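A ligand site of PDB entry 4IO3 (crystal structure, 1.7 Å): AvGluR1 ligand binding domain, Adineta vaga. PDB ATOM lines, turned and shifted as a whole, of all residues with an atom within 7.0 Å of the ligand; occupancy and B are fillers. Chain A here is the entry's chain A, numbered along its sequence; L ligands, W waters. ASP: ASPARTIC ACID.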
ATOM      1  N   SER A  17      -5.488  24.469 -21.794  1.00  0.00           N
ATOM      2  CA  SER A  17      -5.786  25.462 -20.769  1.00  0.00           C
ATOM      3  C   SER A  17      -4.665  26.475 -20.738  1.00  0.00           C
ATOM      4  O   SER A  17      -3.591  26.171 -20.245  1.00  0.00           O
ATOM      5  CB  SER A  17      -5.903  24.830 -19.399  1.00  0.00           C
ATOM      6  OG  SER A  17      -6.253  25.833 -18.466  1.00  0.00           O
ATOM      7  N   SER A  66     -13.751  16.854 -21.249  1.00  0.00           N
ATOM      8  CA  SER A  66     -13.907  17.614 -20.006  1.00  0.00           C
ATOM      9  C   SER A  66     -12.866  17.186 -18.972  1.00  0.00           C
ATOM     10  O   SER A  66     -12.175  16.184 -19.173  1.00  0.00           O
ATOM     11  CB  SER A  66     -15.281  17.400 -19.414  1.00  0.00           C
ATOM     12  OG  SER A  66     -15.427  16.056 -18.969  1.00  0.00           O
ATOM     13  N   TYR A  67     -12.758  17.932 -17.876  1.00  0.00           N
ATOM     14  CA  TYR A  67     -11.787  17.575 -16.841  1.00  0.00           C
ATOM     15  C   TYR A  67     -12.188  16.233 -16.198  1.00  0.00           C
ATOM     16  O   TYR A  67     -11.362  15.335 -15.990  1.00  0.00           O
ATOM     17  CB  TYR A  67     -11.592  18.705 -15.805  1.00  0.00           C
ATOM     18  CG  TYR A  67     -10.649  19.735 -16.352  1.00  0.00           C
ATOM     19  CD1 TYR A  67     -11.064  20.648 -17.319  1.00  0.00           C
ATOM     20  CD2 TYR A  67      -9.321  19.762 -15.949  1.00  0.00           C
ATOM     21  CE1 TYR A  67     -10.200  21.549 -17.850  1.00  0.00           C
ATOM     22  CE2 TYR A  67      -8.447  20.654 -16.481  1.00  0.00           C
ATOM     23  CZ  TYR A  67      -8.876  21.543 -17.435  1.00  0.00           C
ATOM     24  OH  TYR A  67      -7.971  22.436 -17.969  1.00  0.00           O
ATOM     25  N   THR A  68     -13.477  16.060 -15.914  1.00  0.00           N
ATOM     26  CA  THR A  68     -13.911  14.778 -15.401  1.00  0.00           C
ATOM     27  C   THR A  68     -13.688  13.671 -16.427  1.00  0.00           C
ATOM     28  O   THR A  68     -13.316  12.551 -16.083  1.00  0.00           O
ATOM     29  CB  THR A  68     -15.375  14.846 -14.972  1.00  0.00           C
ATOM     30  OG1 THR A  68     -15.463  15.767 -13.888  1.00  0.00           O
ATOM     31  CG2 THR A  68     -15.851  13.465 -14.522  1.00  0.00           C
ATOM     32  N   VAL A  71     -10.035  12.521 -16.307  1.00  0.00           N
ATOM     33  CA  VAL A  71      -9.818  11.637 -15.165  1.00  0.00           C
ATOM     34  C   VAL A  71     -10.385  10.243 -15.471  1.00  0.00           C
ATOM     35  O   VAL A  71      -9.740   9.245 -15.240  1.00  0.00           O
ATOM     36  CB  VAL A  71     -10.465  12.241 -13.895  1.00  0.00           C
ATOM     37  CG1 VAL A  71     -10.505  11.234 -12.763  1.00  0.00           C
ATOM     38  CG2 VAL A  71      -9.747  13.523 -13.446  1.00  0.00           C
ATOM     39  N   ASP A  85      -4.020  21.442 -14.878  1.00  0.00           N
ATOM     40  CA  ASP A  85      -4.760  22.169 -13.882  1.00  0.00           C
ATOM     41  C   ASP A  85      -5.961  21.354 -13.434  1.00  0.00           C
ATOM     42  O   ASP A  85      -7.113  21.763 -13.626  1.00  0.00           O
ATOM     43  CB  ASP A  85      -5.155  23.577 -14.364  1.00  0.00           C
ATOM     44  CG  ASP A  85      -5.865  23.614 -15.732  1.00  0.00           C
ATOM     45  OD1 ASP A  85      -5.773  22.670 -16.538  1.00  0.00           O
ATOM     46  OD2 ASP A  85      -6.522  24.680 -15.991  1.00  0.00           O
ATOM     47  N   ILE A  86      -5.678  20.220 -12.808  1.00  0.00           N
ATOM     48  CA  ILE A  86      -6.667  19.210 -12.486  1.00  0.00           C
ATOM     49  C   ILE A  86      -6.872  19.183 -10.985  1.00  0.00           C
ATOM     50  O   ILE A  86      -5.961  18.821 -10.204  1.00  0.00           O
ATOM     51  CB  ILE A  86      -6.228  17.818 -12.966  1.00  0.00           C
ATOM     52  CG1 ILE A  86      -5.881  17.845 -14.458  1.00  0.00           C
ATOM     53  CG2 ILE A  86      -7.269  16.775 -12.589  1.00  0.00           C
ATOM     54  CD1 ILE A  86      -5.132  16.618 -14.929  1.00  0.00           C
ATOM     55  N   THR A  87      -8.066  19.595 -10.566  1.00  0.00           N
ATOM     56  CA  THR A  87      -8.372  19.709  -9.148  1.00  0.00           C
ATOM     57  C   THR A  87      -8.509  18.348  -8.454  1.00  0.00           C
ATOM     58  O   THR A  87      -9.160  17.442  -8.969  1.00  0.00           O
ATOM     59  CB  THR A  87      -9.652  20.529  -8.947  1.00  0.00           C
ATOM     60  OG1 THR A  87      -9.477  21.787  -9.594  1.00  0.00           O
ATOM     61  CG2 THR A  87      -9.964  20.774  -7.478  1.00  0.00           C
ATOM     62  N   VAL A  88      -7.861  18.235  -7.295  1.00  0.00           N
ATOM     63  CA  VAL A  88      -7.949  17.019  -6.463  1.00  0.00           C
ATOM     64  C   VAL A  88      -9.265  17.086  -5.709  1.00  0.00           C
ATOM     65  O   VAL A  88      -9.493  18.005  -4.938  1.00  0.00           O
ATOM     66  CB  VAL A  88      -6.772  16.934  -5.489  1.00  0.00           C
ATOM     67  CG1 VAL A  88      -6.879  15.699  -4.623  1.00  0.00           C
ATOM     68  CG2 VAL A  88      -5.487  16.916  -6.237  1.00  0.00           C
ATOM     69  N   THR A  89     -10.161  16.152  -5.979  1.00  0.00           N
ATOM     70  CA  THR A  89     -11.418  16.119  -5.278  1.00  0.00           C
ATOM     71  C   THR A  89     -11.697  14.750  -4.689  1.00  0.00           C
ATOM     72  O   THR A  89     -11.184  13.758  -5.166  1.00  0.00           O
ATOM     73  CB  THR A  89     -12.624  16.461  -6.167  1.00  0.00           C
ATOM     74  OG1 THR A  89     -12.837  15.379  -7.102  1.00  0.00           O
ATOM     75  CG2 THR A  89     -12.386  17.775  -6.966  1.00  0.00           C
ATOM     76  N   ARG A  92     -13.168  12.279  -7.248  1.00  0.00           N
ATOM     77  CA  ARG A  92     -12.165  11.769  -8.191  1.00  0.00           C
ATOM     78  C   ARG A  92     -11.247  10.763  -7.506  1.00  0.00           C
ATOM     79  O   ARG A  92     -10.829   9.789  -8.114  1.00  0.00           O
ATOM     80  CB  ARG A  92     -11.354  12.909  -8.825  1.00  0.00           C
ATOM     81  CG  ARG A  92     -12.163  13.732  -9.781  1.00  0.00           C
ATOM     82  CD  ARG A  92     -11.501  15.037 -10.157  1.00  0.00           C
ATOM     83  NE  ARG A  92     -12.329  15.752 -11.131  1.00  0.00           N
ATOM     84  CZ  ARG A  92     -12.002  16.938 -11.637  1.00  0.00           C
ATOM     85  NH1 ARG A  92     -10.870  17.528 -11.281  1.00  0.00           N
ATOM     86  NH2 ARG A  92     -12.834  17.518 -12.517  1.00  0.00           N
ATOM     87  N   ASN A 105      -4.735  25.915  -5.172  1.00  0.00           N
ATOM     88  CA  ASN A 105      -5.757  26.429  -6.087  1.00  0.00           C
ATOM     89  C   ASN A 105      -6.909  26.953  -5.257  1.00  0.00           C
ATOM     90  O   ASN A 105      -7.047  26.622  -4.084  1.00  0.00           O
ATOM     91  CB  ASN A 105      -6.260  25.340  -7.054  1.00  0.00           C
ATOM     92  CG  ASN A 105      -7.304  25.844  -8.060  1.00  0.00           C
ATOM     93  OD1 ASN A 105      -7.035  26.801  -8.819  1.00  0.00           O
ATOM     94  ND2 ASN A 105      -8.486  25.227  -8.075  1.00  0.00           N
ATOM     95  N   MET A 107     -10.985  29.109  -6.345  1.00  0.00           N
ATOM     96  CA  MET A 107     -11.776  29.685  -7.428  1.00  0.00           C
ATOM     97  C   MET A 107     -12.186  31.100  -7.135  1.00  0.00           C
ATOM     98  O   MET A 107     -12.214  31.512  -5.977  1.00  0.00           O
ATOM     99  CB  MET A 107     -13.041  28.863  -7.718  1.00  0.00           C
ATOM    100  CG  MET A 107     -12.723  27.483  -8.305  1.00  0.00           C
ATOM    101  SD  MET A 107     -14.170  26.579  -8.873  1.00  0.00           S
ATOM    102  CE  MET A 107     -14.807  25.986  -7.300  1.00  0.00           C
ATOM    103  N   ARG A 136     -19.215  25.519 -16.150  1.00  0.00           N
ATOM    104  CA  ARG A 136     -18.612  24.555 -17.062  1.00  0.00           C
ATOM    105  C   ARG A 136     -18.808  23.141 -16.540  1.00  0.00           C
ATOM    106  O   ARG A 136     -18.323  22.780 -15.472  1.00  0.00           O
ATOM    107  CB  ARG A 136     -17.153  24.884 -17.253  1.00  0.00           C
ATOM    108  CG  ARG A 136     -16.913  26.083 -18.131  1.00  0.00           C
ATOM    109  CD  ARG A 136     -15.460  26.519 -18.120  1.00  0.00           C
ATOM    110  NE  ARG A 136     -14.617  25.414 -18.533  1.00  0.00           N
ATOM    111  CZ  ARG A 136     -13.497  25.044 -17.930  1.00  0.00           C
ATOM    112  NH1 ARG A 136     -13.078  25.660 -16.829  1.00  0.00           N
ATOM    113  NH2 ARG A 136     -12.817  24.038 -18.427  1.00  0.00           N
ATOM    114  N   GLY A 138     -18.567  19.227 -15.915  1.00  0.00           N
ATOM    115  CA  GLY A 138     -17.427  18.322 -15.799  1.00  0.00           C
ATOM    116  C   GLY A 138     -16.176  18.974 -15.215  1.00  0.00           C
ATOM    117  O   GLY A 138     -15.071  18.488 -15.408  1.00  0.00           O
ATOM    118  N   THR A 139     -16.359  20.089 -14.536  1.00  0.00           N
ATOM    119  CA  THR A 139     -15.325  20.711 -13.743  1.00  0.00           C
ATOM    120  C   THR A 139     -15.661  20.615 -12.264  1.00  0.00           C
ATOM    121  O   THR A 139     -16.797  20.350 -11.843  1.00  0.00           O
ATOM    122  CB  THR A 139     -15.103  22.207 -14.084  1.00  0.00           C
ATOM    123  OG1 THR A 139     -16.248  22.986 -13.696  1.00  0.00           O
ATOM    124  CG2 THR A 139     -14.766  22.412 -15.548  1.00  0.00           C
ATOM    125  N   ALA A 140     -14.638  20.808 -11.437  1.00  0.00           N
ATOM    126  CA  ALA A 140     -14.849  20.807 -10.005  1.00  0.00           C
ATOM    127  C   ALA A 140     -15.853  21.853  -9.567  1.00  0.00           C
ATOM    128  O   ALA A 140     -16.561  21.659  -8.577  1.00  0.00           O
ATOM    129  CB  ALA A 140     -13.508  20.999  -9.288  1.00  0.00           C
ATOM    130  N   GLY A 141     -15.891  22.972 -10.291  1.00  0.00           N
ATOM    131  CA  GLY A 141     -16.787  24.059  -9.978  1.00  0.00           C
ATOM    132  C   GLY A 141     -18.238  23.645 -10.088  1.00  0.00           C
ATOM    133  O   GLY A 141     -19.072  24.218  -9.409  1.00  0.00           O
ATOM    134  N   ARG A 162     -14.294  26.910 -21.922  1.00  0.00           N
ATOM    135  CA  ARG A 162     -13.955  28.245 -21.459  1.00  0.00           C
ATOM    136  C   ARG A 162     -14.400  29.269 -22.511  1.00  0.00           C
ATOM    137  O   ARG A 162     -14.883  30.353 -22.164  1.00  0.00           O
ATOM    138  CB  ARG A 162     -12.458  28.361 -21.167  1.00  0.00           C
ATOM    139  CG  ARG A 162     -12.035  27.551 -19.975  1.00  0.00           C
ATOM    140  CD  ARG A 162     -10.594  27.779 -19.638  1.00  0.00           C
ATOM    141  NE  ARG A 162     -10.162  26.833 -18.613  1.00  0.00           N
ATOM    142  CZ  ARG A 162      -9.602  25.643 -18.853  1.00  0.00           C
ATOM    143  NH1 ARG A 162      -9.355  25.200 -20.087  1.00  0.00           N
ATOM    144  NH2 ARG A 162      -9.285  24.890 -17.828  1.00  0.00           N
ATOM    145  N   PHE A 178     -17.704  30.675 -12.542  1.00  0.00           N
ATOM    146  CA  PHE A 178     -16.579  30.392 -11.646  1.00  0.00           C
ATOM    147  C   PHE A 178     -15.350  29.992 -12.432  1.00  0.00           C
ATOM    148  O   PHE A 178     -15.463  29.289 -13.446  1.00  0.00           O
ATOM    149  CB  PHE A 178     -16.890  29.212 -10.717  1.00  0.00           C
ATOM    150  CG  PHE A 178     -18.129  29.363  -9.876  1.00  0.00           C
ATOM    151  CD1 PHE A 178     -18.663  30.586  -9.559  1.00  0.00           C
ATOM    152  CD2 PHE A 178     -18.716  28.218  -9.342  1.00  0.00           C
ATOM    153  CE1 PHE A 178     -19.802  30.687  -8.761  1.00  0.00           C
ATOM    154  CE2 PHE A 178     -19.836  28.298  -8.544  1.00  0.00           C
ATOM    155  CZ  PHE A 178     -20.397  29.516  -8.246  1.00  0.00           C
ATOM    156  N   MET A 179     -14.169  30.359 -11.950  1.00  0.00           N
ATOM    157  CA  MET A 179     -12.945  29.951 -12.613  1.00  0.00           C
ATOM    158  C   MET A 179     -11.842  29.763 -11.595  1.00  0.00           C
ATOM    159  O   MET A 179     -11.756  30.520 -10.637  1.00  0.00           O
ATOM    160  CB  MET A 179     -12.571  31.046 -13.612  1.00  0.00           C
ATOM    161  CG  MET A 179     -11.669  30.629 -14.701  1.00  0.00           C
ATOM    162  SD  MET A 179     -11.504  31.892 -15.999  1.00  0.00           S
ATOM    163  CE  MET A 179     -10.152  31.047 -16.809  1.00  0.00           C
ATOM    164  N   ASP A 180     -10.957  28.805 -11.838  1.00  0.00           N
ATOM    165  CA  ASP A 180      -9.748  28.666 -11.028  1.00  0.00           C
ATOM    166  C   ASP A 180      -8.910  29.957 -11.065  1.00  0.00           C
ATOM    167  O   ASP A 180      -8.779  30.596 -12.105  1.00  0.00           O
ATOM    168  CB  ASP A 180      -8.856  27.541 -11.580  1.00  0.00           C
ATOM    169  CG  ASP A 180      -9.445  26.155 -11.428  1.00  0.00           C
ATOM    170  OD1 ASP A 180     -10.221  25.866 -10.475  1.00  0.00           O
ATOM    171  OD2 ASP A 180      -9.060  25.283 -12.260  1.00  0.00           O
ATOM    172  N   THR A 183      -5.599  30.568 -13.828  1.00  0.00           N
ATOM    173  CA  THR A 183      -6.048  30.872 -15.183  1.00  0.00           C
ATOM    174  C   THR A 183      -6.994  32.086 -15.250  1.00  0.00           C
ATOM    175  O   THR A 183      -7.003  32.833 -16.232  1.00  0.00           O
ATOM    176  CB  THR A 183      -6.676  29.625 -15.866  1.00  0.00           C
ATOM    177  OG1 THR A 183      -7.713  29.091 -15.025  1.00  0.00           O
ATOM    178  CG2 THR A 183      -5.609  28.577 -16.113  1.00  0.00           C
ATOM    179  N   THR A 206      -6.238  21.809  -4.344  1.00  0.00           N
ATOM    180  CA  THR A 206      -4.925  21.636  -4.954  1.00  0.00           C
ATOM    181  C   THR A 206      -5.040  21.059  -6.338  1.00  0.00           C
ATOM    182  O   THR A 206      -6.090  20.490  -6.692  1.00  0.00           O
ATOM    183  CB  THR A 206      -4.086  20.667  -4.120  1.00  0.00           C
ATOM    184  OG1 THR A 206      -4.810  19.444  -3.927  1.00  0.00           O
ATOM    185  CG2 THR A 206      -3.793  21.272  -2.755  1.00  0.00           C
ATOM    186  N   PHE A 207      -3.985  21.201  -7.130  1.00  0.00           N
ATOM    187  CA  PHE A 207      -3.855  20.495  -8.386  1.00  0.00           C
ATOM    188  C   PHE A 207      -2.846  19.369  -8.160  1.00  0.00           C
ATOM    189  O   PHE A 207      -1.817  19.574  -7.518  1.00  0.00           O
ATOM    190  CB  PHE A 207      -3.309  21.375  -9.514  1.00  0.00           C
ATOM    191  CG  PHE A 207      -4.204  22.498  -9.947  1.00  0.00           C
ATOM    192  CD1 PHE A 207      -5.578  22.375  -9.889  1.00  0.00           C
ATOM    193  CD2 PHE A 207      -3.656  23.635 -10.490  1.00  0.00           C
ATOM    194  CE1 PHE A 207      -6.374  23.418 -10.320  1.00  0.00           C
ATOM    195  CE2 PHE A 207      -4.440  24.689 -10.927  1.00  0.00           C
ATOM    196  CZ  PHE A 207      -5.795  24.565 -10.865  1.00  0.00           C
HETATM  197  N   ASP L   1      -9.500  22.658 -12.290  1.00  0.00           N
HETATM  198  CA  ASP L   1     -10.833  22.282 -12.827  1.00  0.00           C
HETATM  199  C   ASP L   1     -11.049  20.787 -12.715  1.00  0.00           C
HETATM  200  O   ASP L   1     -10.092  19.997 -12.485  1.00  0.00           O
HETATM  201  CB  ASP L   1     -10.987  22.680 -14.308  1.00  0.00           C
HETATM  202  CG  ASP L   1     -11.309  24.143 -14.489  1.00  0.00           C
HETATM  203  OD1 ASP L   1     -10.880  24.737 -15.539  1.00  0.00           O
HETATM  204  OD2 ASP L   1     -11.999  24.713 -13.612  1.00  0.00           O
HETATM  205  OXT ASP L   1     -12.196  20.346 -12.871  1.00  0.00           O
HETATM  206  O   HOH W   1     -11.755  27.106 -14.014  1.00  0.00           O
HETATM  207  O   HOH W   2     -13.561  24.161 -11.503  1.00  0.00           O
HETATM  208  O   HOH W   3      -9.867  27.509 -15.942  1.00  0.00           O
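The guanidinium group (NH1) of Arg 92 is in salt-bridge range of an oxygen (O) of the ligand (2.9 Å).
The side-chain hydroxyl (OG1) of Thr 87 sits at hydrogen-bond distance from a nitrogen (N) of the ligand.
OD1 of the ligand lies within salt-bridge range of NH1 of Arg 136 (2.7 Å).
NH2 of Arg 162 is in salt-bridge range of OD1 of the ligand, at 2.8 Å.
N of Thr 87 is in hydrogen-bond range of O of the ligand, at 2.8 Å.
OD2 of Asp 180 is in salt-bridge range of N of the ligand.
An oxygen (OXT) of the ligand is in hydrogen-bond range of the backbone NH (N) of Ala 140 (2.9 Å).
A nitrogen (N) of the ligand is in hydrogen-bond range of the backbone carbonyl oxygen of Asp 85 (2.9 Å).
Water W1 lies within hydrogen-bond range of OD2 of the ligand (2.4 Å), N of Asp 180 (2.9 Å) and NH1 of Arg 136 (3.4 Å).
Water W2 lies within hydrogen-bond range of an oxygen (OD2) of the ligand (2.7 Å), the backbone NH (N) of Gly 141 (2.9 Å) and the side-chain sulfur (SD) of Met 107 (3.6 Å).
Water W3 lies within hydrogen-bond range of the guanidinium group (NE) of Arg 162 (2.8 Å), the side-chain hydroxyl (OG1) of Thr 183 (2.8 Å) and an oxygen (OD1) of the ligand (3.0 Å).
OH of Tyr 67 is in hydrogen-bond range of NH2 of Arg 162 (2.8 Å).
NH2 of Arg 162 is in salt-bridge range of OD2 of Asp 85.
N of Tyr 67 sits at hydrogen-bond distance from O of Gly 138 (3.4 Å).
NH2 of Arg 162 is in hydrogen-bond range of OG of Ser 17 (3.2 Å).
OG1 of Thr 139 sits close to N of Gly 141, at 3.4 Å.
O of Arg 136 lies within hydrogen-bond range of OG1 of Thr 139, at 2.7 Å.
OD1 of Asp 85 sits at hydrogen-bond distance from OH of Tyr 67.
O of Thr 87 lies within hydrogen-bond range of NH1 of Arg 92 (2.9 Å).
Tyr 67 touches the ligand.
CA of Ile 86 touches O of the ligand, at 3.5 Å.
CA of Thr 139 touches OXT of the ligand (3.3 Å).
Phe 207 touches the ligand (CE1 to N, 3.8 Å).
Hydrophobic or aromatic side chains within 4 Å of the ligand: Tyr 67, Ala 140 and Phe 207.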
